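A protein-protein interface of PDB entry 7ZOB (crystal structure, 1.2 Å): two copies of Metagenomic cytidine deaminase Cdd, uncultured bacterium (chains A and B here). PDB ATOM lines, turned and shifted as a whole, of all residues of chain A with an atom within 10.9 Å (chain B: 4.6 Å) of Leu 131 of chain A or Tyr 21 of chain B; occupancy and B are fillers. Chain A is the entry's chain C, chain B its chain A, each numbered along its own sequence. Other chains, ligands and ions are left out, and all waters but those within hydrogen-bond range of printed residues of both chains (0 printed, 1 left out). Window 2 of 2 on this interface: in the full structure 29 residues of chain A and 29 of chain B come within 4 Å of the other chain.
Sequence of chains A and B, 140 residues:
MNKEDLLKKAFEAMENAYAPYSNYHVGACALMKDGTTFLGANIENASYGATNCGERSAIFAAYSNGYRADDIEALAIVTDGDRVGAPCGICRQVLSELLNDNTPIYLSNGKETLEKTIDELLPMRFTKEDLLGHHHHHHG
Printed residues of chain A that touch a printed residue of chain B: Gln 93, Val 94, Glu 97, Phe 126, Thr 127, Lys 128 and Leu 131. Hydrophobic or aromatic side chains of chain A within 4 Å of the printed part of chain B: Phe 126 and Leu 131. Among the printed residues, 12 pairs touch across the chains. Among the printed residues, no Asp or Glu carboxylate lies within 4 Å of a Lys or Arg side-chain nitrogen of the other chain.
Among the printed residues, merely in contact across the chains: Val 94 of chain A with Asn 45 of chain B, Glu 97 of chain A with Asn 45 of chain B, Phe 126 of chain A with Ala 46 of chain B, Thr 127 of chain A with Ala 46 of chain B, Lys 128 of chain A with Tyr 21 of chain B, Lys 128 of chain A with Ala 46 of chain B, Leu 131 of chain A with Tyr 21 of chain B, Leu 131 of chain A with Ala 46 of chain B and Leu 131 of chain A with Tyr 48 of chain B.
The side-chain carboxylate (OE2) of Glu 97 of chain A is in hydrogen-bond range of the side-chain hydroxyl (OH) of Tyr 21 of chain B (2.7 Å). The side-chain amide nitrogen (ND2) of Asn 45 of chain B lies within hydrogen-bond range of the backbone carbonyl oxygen (O) of Gln 93 of chain A. The backbone NH (N) of Ala 46 of chain B sits at hydrogen-bond distance from the side-chain carboxylate (OE1) of Glu 97 of chain A (2.9 Å).
Leu 131 of chain A touches just these residues of chain B: Tyr 21, Ala 46 and Tyr 48. Of the printed residues of chain A, Tyr 21 of chain B touches Glu 97 (2.7 Å), Lys 128 (3.2 Å) and Leu 131 (3.7 Å). No residue of chain A comes within 4 Å of Ala 19 of chain B. No residue of chain A comes within 4 Å of Glu 44 of chain B. Of the printed residues of chain A, Asn 45 of chain B touches Gln 93 (3.0 Å), Val 94 (3.5 Å) and Glu 97 (3.4 Å). Of the printed residues of chain B, Gln 93 of chain A touches Asn 45. Of the printed residues of chain B, Phe 126 of chain A touches Ala 46. Printed residues of chain B within 4 Å of Glu 97 of chain A: Tyr 21 (2.7 Å), Asn 45 (3.4 Å) and Ala 46 (2.9 Å). Of the printed residues of chain B, Thr 127 of chain A touches Ala 46 (3.8 Å). His 134 of chain A touches none of the printed residues of chain B. The nearest printed residue of chain B that does not touch Leu 131 of chain A is Asn 45 of chain B (5.4 Å). The nearest printed residue of chain A that does not touch Tyr 21 of chain B is Leu 132 of chain A (4.02 Å).
The backbone NH (N) of Tyr 21 of chain B is in hydrogen-bond range of the side-chain carboxylate (OE1) of Glu 44 of chain B, at 3.0 Å. OH of Tyr 21 of chain B lies close to N of Ala 46 of chain B. N of Glu 129 of chain A sits close to OG1 of Thr 127 of chain A, at 3.3 Å. OD2 of Asp 130 of chain A is in hydrogen-bond range of N of Thr 127 of chain A, 3.0 Å away.
No position is printed for both chains. Of the 12 pairs that touch across the chains among the printed residues, none has its exchanged pair printed and touching as well.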
ATOM      1  N   TYR A  63     -17.700  13.593 -39.126  1.00  0.00           N
ATOM      2  CA  TYR A  63     -18.525  12.406 -39.307  1.00  0.00           C
ATOM      3  C   TYR A  63     -19.912  12.772 -39.814  1.00  0.00           C
ATOM      4  O   TYR A  63     -20.499  12.032 -40.614  1.00  0.00           O
ATOM      5  CB  TYR A  63     -18.619  11.631 -37.991  1.00  0.00           C
ATOM      6  CG  TYR A  63     -17.551  10.576 -37.828  1.00  0.00           C
ATOM      7  CD1 TYR A  63     -16.210  10.906 -37.681  1.00  0.00           C
ATOM      8  CD2 TYR A  63     -17.890   9.211 -37.830  1.00  0.00           C
ATOM      9  CE1 TYR A  63     -15.232   9.934 -37.557  1.00  0.00           C
ATOM     10  CE2 TYR A  63     -16.922   8.242 -37.684  1.00  0.00           C
ATOM     11  CZ  TYR A  63     -15.604   8.600 -37.564  1.00  0.00           C
ATOM     12  OH  TYR A  63     -14.680   7.590 -37.444  1.00  0.00           O
ATOM     13  N   GLN A  93     -12.234   8.696 -25.114  1.00  0.00           N
ATOM     14  CA  GLN A  93     -13.159   7.604 -25.402  1.00  0.00           C
ATOM     15  C   GLN A  93     -13.773   7.764 -26.793  1.00  0.00           C
ATOM     16  O   GLN A  93     -13.910   6.785 -27.536  1.00  0.00           O
ATOM     17  CB  GLN A  93     -14.253   7.555 -24.333  1.00  0.00           C
ATOM     18  CG  GLN A  93     -15.193   6.384 -24.474  1.00  0.00           C
ATOM     19  CD  GLN A  93     -14.474   5.068 -24.395  1.00  0.00           C
ATOM     20  OE1 GLN A  93     -13.647   4.857 -23.484  1.00  0.00           O
ATOM     21  NE2 GLN A  93     -14.806   4.138 -25.303  1.00  0.00           N
ATOM     22  N   VAL A  94     -14.137   8.995 -27.165  1.00  0.00           N
ATOM     23  CA  VAL A  94     -14.663   9.251 -28.502  1.00  0.00           C
ATOM     24  C   VAL A  94     -13.600   8.991 -29.571  1.00  0.00           C
ATOM     25  O   VAL A  94     -13.854   8.293 -30.568  1.00  0.00           O
ATOM     26  CB  VAL A  94     -15.247  10.673 -28.588  1.00  0.00           C
ATOM     27  CG1 VAL A  94     -15.554  11.026 -30.051  1.00  0.00           C
ATOM     28  CG2 VAL A  94     -16.478  10.766 -27.713  1.00  0.00           C
ATOM     29  N   LEU A  95     -12.398   9.549 -29.394  1.00  0.00           N
ATOM     30  CA  LEU A  95     -11.356   9.369 -30.401  1.00  0.00           C
ATOM     31  C   LEU A  95     -10.937   7.909 -30.528  1.00  0.00           C
ATOM     32  O   LEU A  95     -10.535   7.482 -31.626  1.00  0.00           O
ATOM     33  CB  LEU A  95     -10.167  10.273 -30.091  1.00  0.00           C
ATOM     34  CG  LEU A  95     -10.461  11.769 -30.065  1.00  0.00           C
ATOM     35  CD1 LEU A  95      -9.201  12.538 -29.721  1.00  0.00           C
ATOM     36  CD2 LEU A  95     -11.042  12.208 -31.397  1.00  0.00           C
ATOM     37  N   SER A  96     -11.026   7.131 -29.445  1.00  0.00           N
ATOM     38  CA  SER A  96     -10.726   5.700 -29.513  1.00  0.00           C
ATOM     39  C   SER A  96     -11.623   5.005 -30.520  1.00  0.00           C
ATOM     40  O   SER A  96     -11.194   4.046 -31.182  1.00  0.00           O
ATOM     41  CB  SER A  96     -10.933   5.090 -28.123  1.00  0.00           C
ATOM     42  OG  SER A  96     -10.696   3.691 -28.119  1.00  0.00           O
ATOM     43  N   GLU A  97     -12.824   5.422 -30.653  1.00  0.00           N
ATOM     44  CA  GLU A  97     -13.800   4.885 -31.584  1.00  0.00           C
ATOM     45  C   GLU A  97     -13.647   5.475 -32.995  1.00  0.00           C
ATOM     46  O   GLU A  97     -13.770   4.761 -33.983  1.00  0.00           O
ATOM     47  CB  GLU A  97     -15.217   5.124 -31.067  1.00  0.00           C
ATOM     48  CG  GLU A  97     -16.329   4.619 -31.974  1.00  0.00           C
ATOM     49  CD  GLU A  97     -17.147   3.505 -31.353  1.00  0.00           C
ATOM     50  OE1 GLU A  97     -16.976   3.230 -30.155  1.00  0.00           O
ATOM     51  OE2 GLU A  97     -17.972   2.912 -32.066  1.00  0.00           O
ATOM     52  N   LEU A  98     -13.387   6.778 -33.085  1.00  0.00           N
ATOM     53  CA  LEU A  98     -13.567   7.483 -34.348  1.00  0.00           C
ATOM     54  C   LEU A  98     -12.277   7.729 -35.121  1.00  0.00           C
ATOM     55  O   LEU A  98     -12.352   8.119 -36.294  1.00  0.00           O
ATOM     56  CB  LEU A  98     -14.302   8.810 -34.103  1.00  0.00           C
ATOM     57  CG  LEU A  98     -15.668   8.747 -33.418  1.00  0.00           C
ATOM     58  CD1 LEU A  98     -16.287  10.105 -33.420  1.00  0.00           C
ATOM     59  CD2 LEU A  98     -16.586   7.753 -34.137  1.00  0.00           C
ATOM     60  N   ARG A 125      -8.124   0.002 -23.919  1.00  0.00           N
ATOM     61  CA  ARG A 125      -9.320   0.580 -24.526  1.00  0.00           C
ATOM     62  C   ARG A 125     -10.484  -0.395 -24.515  1.00  0.00           C
ATOM     63  O   ARG A 125     -10.311  -1.580 -24.780  1.00  0.00           O
ATOM     64  CB  ARG A 125      -9.013   0.988 -25.968  1.00  0.00           C
ATOM     65  CG  ARG A 125      -7.965   2.088 -25.999  1.00  0.00           C
ATOM     66  CD  ARG A 125      -7.223   2.188 -27.333  1.00  0.00           C
ATOM     67  NE  ARG A 125      -8.115   2.551 -28.422  1.00  0.00           N
ATOM     68  CZ  ARG A 125      -7.764   2.532 -29.702  1.00  0.00           C
ATOM     69  NH1 ARG A 125      -6.546   2.160 -30.082  1.00  0.00           N
ATOM     70  NH2 ARG A 125      -8.665   2.850 -30.619  1.00  0.00           N
ATOM     71  N   PHE A 126     -11.675   0.127 -24.216  1.00  0.00           N
ATOM     72  CA  PHE A 126     -12.915  -0.604 -24.434  1.00  0.00           C
ATOM     73  C   PHE A 126     -13.431  -0.288 -25.829  1.00  0.00           C
ATOM     74  O   PHE A 126     -13.760   0.876 -26.117  1.00  0.00           O
ATOM     75  CB  PHE A 126     -13.970  -0.227 -23.402  1.00  0.00           C
ATOM     76  CG  PHE A 126     -15.259  -0.989 -23.564  1.00  0.00           C
ATOM     77  CD1 PHE A 126     -15.337  -2.313 -23.167  1.00  0.00           C
ATOM     78  CD2 PHE A 126     -16.395  -0.383 -24.080  1.00  0.00           C
ATOM     79  CE1 PHE A 126     -16.502  -3.028 -23.292  1.00  0.00           C
ATOM     80  CE2 PHE A 126     -17.582  -1.101 -24.219  1.00  0.00           C
ATOM     81  CZ  PHE A 126     -17.628  -2.425 -23.819  1.00  0.00           C
ATOM     82  N   THR A 127     -13.534  -1.307 -26.670  1.00  0.00           N
ATOM     83  CA  THR A 127     -13.741  -1.057 -28.084  1.00  0.00           C
ATOM     84  C   THR A 127     -15.098  -1.575 -28.542  1.00  0.00           C
ATOM     85  O   THR A 127     -15.794  -2.333 -27.854  1.00  0.00           O
ATOM     86  CB  THR A 127     -12.691  -1.790 -28.909  1.00  0.00           C
ATOM     87  OG1 THR A 127     -12.881  -3.195 -28.703  1.00  0.00           O
ATOM     88  CG2 THR A 127     -11.271  -1.403 -28.526  1.00  0.00           C
ATOM     89  N   LYS A 128     -15.445  -1.174 -29.766  1.00  0.00           N
ATOM     90  CA  LYS A 128     -16.630  -1.700 -30.426  1.00  0.00           C
ATOM     91  C   LYS A 128     -16.647  -3.220 -30.383  1.00  0.00           C
ATOM     92  O   LYS A 128     -17.677  -3.829 -30.085  1.00  0.00           O
ATOM     93  CB  LYS A 128     -16.650  -1.216 -31.878  1.00  0.00           C
ATOM     94  CG  LYS A 128     -17.826  -1.786 -32.693  1.00  0.00           C
ATOM     95  CD  LYS A 128     -17.726  -1.474 -34.185  1.00  0.00           C
ATOM     96  CE  LYS A 128     -18.015  -0.020 -34.414  1.00  0.00           C
ATOM     97  NZ  LYS A 128     -17.737   0.425 -35.829  1.00  0.00           N
ATOM     98  N   GLU A 129     -15.509  -3.854 -30.662  1.00  0.00           N
ATOM     99  CA  GLU A 129     -15.495  -5.313 -30.674  1.00  0.00           C
ATOM    100  C   GLU A 129     -15.699  -5.904 -29.289  1.00  0.00           C
ATOM    101  O   GLU A 129     -16.309  -6.971 -29.164  1.00  0.00           O
ATOM    102  CB  GLU A 129     -14.221  -5.849 -31.318  1.00  0.00           C
ATOM    103  CG  GLU A 129     -14.323  -5.907 -32.816  1.00  0.00           C
ATOM    104  N   ASP A 130     -15.215  -5.244 -28.233  1.00  0.00           N
ATOM    105  CA  ASP A 130     -15.506  -5.751 -26.896  1.00  0.00           C
ATOM    106  C   ASP A 130     -17.006  -5.787 -26.639  1.00  0.00           C
ATOM    107  O   ASP A 130     -17.524  -6.732 -26.032  1.00  0.00           O
ATOM    108  CB  ASP A 130     -14.832  -4.898 -25.824  1.00  0.00           C
ATOM    109  CG  ASP A 130     -13.305  -5.020 -25.819  1.00  0.00           C
ATOM    110  OD1 ASP A 130     -12.803  -6.153 -25.966  1.00  0.00           O
ATOM    111  OD2 ASP A 130     -12.608  -3.985 -25.600  1.00  0.00           O
ATOM    112  N   LEU A 131     -17.728  -4.764 -27.091  1.00  0.00           N
ATOM    113  CA  LEU A 131     -19.169  -4.739 -26.885  1.00  0.00           C
ATOM    114  C   LEU A 131     -19.884  -5.706 -27.826  1.00  0.00           C
ATOM    115  O   LEU A 131     -20.719  -6.501 -27.387  1.00  0.00           O
ATOM    116  CB  LEU A 131     -19.673  -3.317 -27.088  1.00  0.00           C
ATOM    117  CG  LEU A 131     -21.193  -3.154 -26.984  1.00  0.00           C
ATOM    118  CD1 LEU A 131     -21.750  -3.772 -25.715  1.00  0.00           C
ATOM    119  CD2 LEU A 131     -21.573  -1.685 -27.042  1.00  0.00           C
ATOM    120  N   LEU A 132     -19.591  -5.632 -29.128  1.00  0.00           N
ATOM    121  CA  LEU A 132     -20.324  -6.460 -30.082  1.00  0.00           C
ATOM    122  C   LEU A 132     -20.077  -7.939 -29.836  1.00  0.00           C
ATOM    123  O   LEU A 132     -20.938  -8.769 -30.160  1.00  0.00           O
ATOM    124  CB  LEU A 132     -19.956  -6.071 -31.516  1.00  0.00           C
ATOM    125  CG  LEU A 132     -20.348  -4.657 -31.952  1.00  0.00           C
ATOM    126  CD1 LEU A 132     -20.000  -4.448 -33.430  1.00  0.00           C
ATOM    127  CD2 LEU A 132     -21.811  -4.347 -31.709  1.00  0.00           C
ATOM    128  N   GLY A 133     -18.923  -8.301 -29.280  1.00  0.00           N
ATOM    129  CA  GLY A 133     -18.606  -9.697 -29.018  1.00  0.00           C
ATOM    130  C   GLY A 133     -19.121 -10.245 -27.710  1.00  0.00           C
ATOM    131  O   GLY A 133     -18.963 -11.440 -27.430  1.00  0.00           O
ATOM    132  N   HIS A 134     -19.773  -9.420 -26.905  1.00  0.00           N
ATOM    133  CA  HIS A 134     -20.230  -9.819 -25.584  1.00  0.00           C
ATOM    134  C   HIS A 134     -21.362 -10.828 -25.670  1.00  0.00           C
ATOM    135  O   HIS A 134     -22.346 -10.583 -26.366  1.00  0.00           O
ATOM    136  CB  HIS A 134     -20.675  -8.566 -24.817  1.00  0.00           C
ATOM    137  CG  HIS A 134     -21.140  -8.843 -23.426  1.00  0.00           C
ATOM    138  ND1 HIS A 134     -22.445  -8.647 -23.024  1.00  0.00           N
ATOM    139  CD2 HIS A 134     -20.474  -9.294 -22.340  1.00  0.00           C
ATOM    140  CE1 HIS A 134     -22.563  -8.971 -21.750  1.00  0.00           C
ATOM    141  NE2 HIS A 134     -21.381  -9.360 -21.310  1.00  0.00           N
ATOM    142  N   ALA B  19     -24.256   5.003 -36.197  1.00  0.00           N
ATOM    143  CA  ALA B  19     -25.052   4.388 -35.140  1.00  0.00           C
ATOM    144  C   ALA B  19     -24.890   2.871 -35.199  1.00  0.00           C
ATOM    145  O   ALA B  19     -25.853   2.134 -35.424  1.00  0.00           O
ATOM    146  CB  ALA B  19     -26.520   4.801 -35.252  1.00  0.00           C
ATOM    147  N   PRO B  20     -23.677   2.364 -34.968  1.00  0.00           N
ATOM    148  CA  PRO B  20     -23.461   0.911 -35.072  1.00  0.00           C
ATOM    149  C   PRO B  20     -24.189   0.107 -34.017  1.00  0.00           C
ATOM    150  O   PRO B  20     -24.334  -1.103 -34.183  1.00  0.00           O
ATOM    151  CB  PRO B  20     -21.945   0.759 -34.902  1.00  0.00           C
ATOM    152  CG  PRO B  20     -21.462   2.014 -34.401  1.00  0.00           C
ATOM    153  CD  PRO B  20     -22.421   3.088 -34.710  1.00  0.00           C
ATOM    154  N   TYR B  21     -24.605   0.730 -32.914  1.00  0.00           N
ATOM    155  CA  TYR B  21     -25.192   0.009 -31.794  1.00  0.00           C
ATOM    156  C   TYR B  21     -26.708  -0.003 -31.885  1.00  0.00           C
ATOM    157  O   TYR B  21     -27.317  -1.068 -31.875  1.00  0.00           O
ATOM    158  CB  TYR B  21     -24.666   0.547 -30.444  1.00  0.00           C
ATOM    159  CG  TYR B  21     -23.143   0.603 -30.487  1.00  0.00           C
ATOM    160  CD1 TYR B  21     -22.374  -0.568 -30.464  1.00  0.00           C
ATOM    161  CD2 TYR B  21     -22.479   1.818 -30.668  1.00  0.00           C
ATOM    162  CE1 TYR B  21     -20.992  -0.523 -30.584  1.00  0.00           C
ATOM    163  CE2 TYR B  21     -21.108   1.872 -30.792  1.00  0.00           C
ATOM    164  CZ  TYR B  21     -20.380   0.700 -30.754  1.00  0.00           C
ATOM    165  OH  TYR B  21     -19.020   0.724 -30.875  1.00  0.00           O
ATOM    166  N   SER B  22     -27.336   1.157 -32.029  1.00  0.00           N
ATOM    167  CA  SER B  22     -28.793   1.208 -32.094  1.00  0.00           C
ATOM    168  C   SER B  22     -29.346   1.032 -33.492  1.00  0.00           C
ATOM    169  O   SER B  22     -30.518   0.661 -33.633  1.00  0.00           O
ATOM    170  CB  SER B  22     -29.327   2.548 -31.592  1.00  0.00           C
ATOM    171  OG  SER B  22     -29.025   3.574 -32.520  1.00  0.00           O
ATOM    172  N   ASN B  23     -28.558   1.345 -34.515  1.00  0.00           N
ATOM    173  CA  ASN B  23     -29.039   1.467 -35.887  1.00  0.00           C
ATOM    174  C   ASN B  23     -30.128   2.535 -36.057  1.00  0.00           C
ATOM    175  O   ASN B  23     -30.834   2.552 -37.054  1.00  0.00           O
ATOM    176  CB  ASN B  23     -29.487   0.128 -36.485  1.00  0.00           C
ATOM    177  CG  ASN B  23     -29.500   0.163 -37.997  1.00  0.00           C
ATOM    178  OD1 ASN B  23     -28.528   0.586 -38.629  1.00  0.00           O
ATOM    179  ND2 ASN B  23     -30.623  -0.228 -38.584  1.00  0.00           N
ATOM    180  N   GLU B  44     -22.603   7.451 -32.268  1.00  0.00           N
ATOM    181  CA  GLU B  44     -22.578   6.577 -31.111  1.00  0.00           C
ATOM    182  C   GLU B  44     -21.153   6.187 -30.717  1.00  0.00           C
ATOM    183  O   GLU B  44     -20.185   6.403 -31.470  1.00  0.00           O
ATOM    184  CB  GLU B  44     -23.469   5.356 -31.332  1.00  0.00           C
ATOM    185  CG  GLU B  44     -24.894   5.773 -31.550  1.00  0.00           C
ATOM    186  CD  GLU B  44     -25.883   4.647 -31.720  1.00  0.00           C
ATOM    187  OE1 GLU B  44     -25.500   3.486 -32.011  1.00  0.00           O
ATOM    188  OE2 GLU B  44     -27.097   4.969 -31.564  1.00  0.00           O
ATOM    189  N   ASN B  45     -21.032   5.617 -29.519  1.00  0.00           N
ATOM    190  CA  ASN B  45     -19.769   5.131 -28.980  1.00  0.00           C
ATOM    191  C   ASN B  45     -20.050   3.849 -28.209  1.00  0.00           C
ATOM    192  O   ASN B  45     -21.114   3.702 -27.584  1.00  0.00           O
ATOM    193  CB  ASN B  45     -19.172   6.167 -28.001  1.00  0.00           C
ATOM    194  CG  ASN B  45     -17.721   5.874 -27.654  1.00  0.00           C
ATOM    195  OD1 ASN B  45     -17.414   5.135 -26.716  1.00  0.00           O
ATOM    196  ND2 ASN B  45     -16.805   6.471 -28.424  1.00  0.00           N
ATOM    197  N   ALA B  46     -19.061   2.953 -28.218  1.00  0.00           N
ATOM    198  CA  ALA B  46     -19.171   1.713 -27.464  1.00  0.00           C
ATOM    199  C   ALA B  46     -19.454   1.981 -25.989  1.00  0.00           C
ATOM    200  O   ALA B  46     -20.139   1.173 -25.341  1.00  0.00           O
ATOM    201  CB  ALA B  46     -17.915   0.876 -27.643  1.00  0.00           C
ATOM    202  N   TYR B  48     -21.786   4.001 -24.176  1.00  0.00           N
ATOM    203  CA  TYR B  48     -22.972   4.674 -24.707  1.00  0.00           C
ATOM    204  C   TYR B  48     -23.071   6.126 -24.281  1.00  0.00           C
ATOM    205  O   TYR B  48     -23.530   6.961 -25.056  1.00  0.00           O
ATOM    206  CB  TYR B  48     -24.251   3.961 -24.312  1.00  0.00           C
ATOM    207  CG  TYR B  48     -24.584   2.709 -25.115  1.00  0.00           C
ATOM    208  CD1 TYR B  48     -23.723   2.179 -26.081  1.00  0.00           C
ATOM    209  CD2 TYR B  48     -25.787   2.041 -24.891  1.00  0.00           C
ATOM    210  CE1 TYR B  48     -24.083   1.029 -26.794  1.00  0.00           C
ATOM    211  CE2 TYR B  48     -26.135   0.904 -25.579  1.00  0.00           C
ATOM    212  CZ  TYR B  48     -25.294   0.403 -26.540  1.00  0.00           C
ATOM    213  OH  TYR B  48     -25.639  -0.746 -27.208  1.00  0.00           O
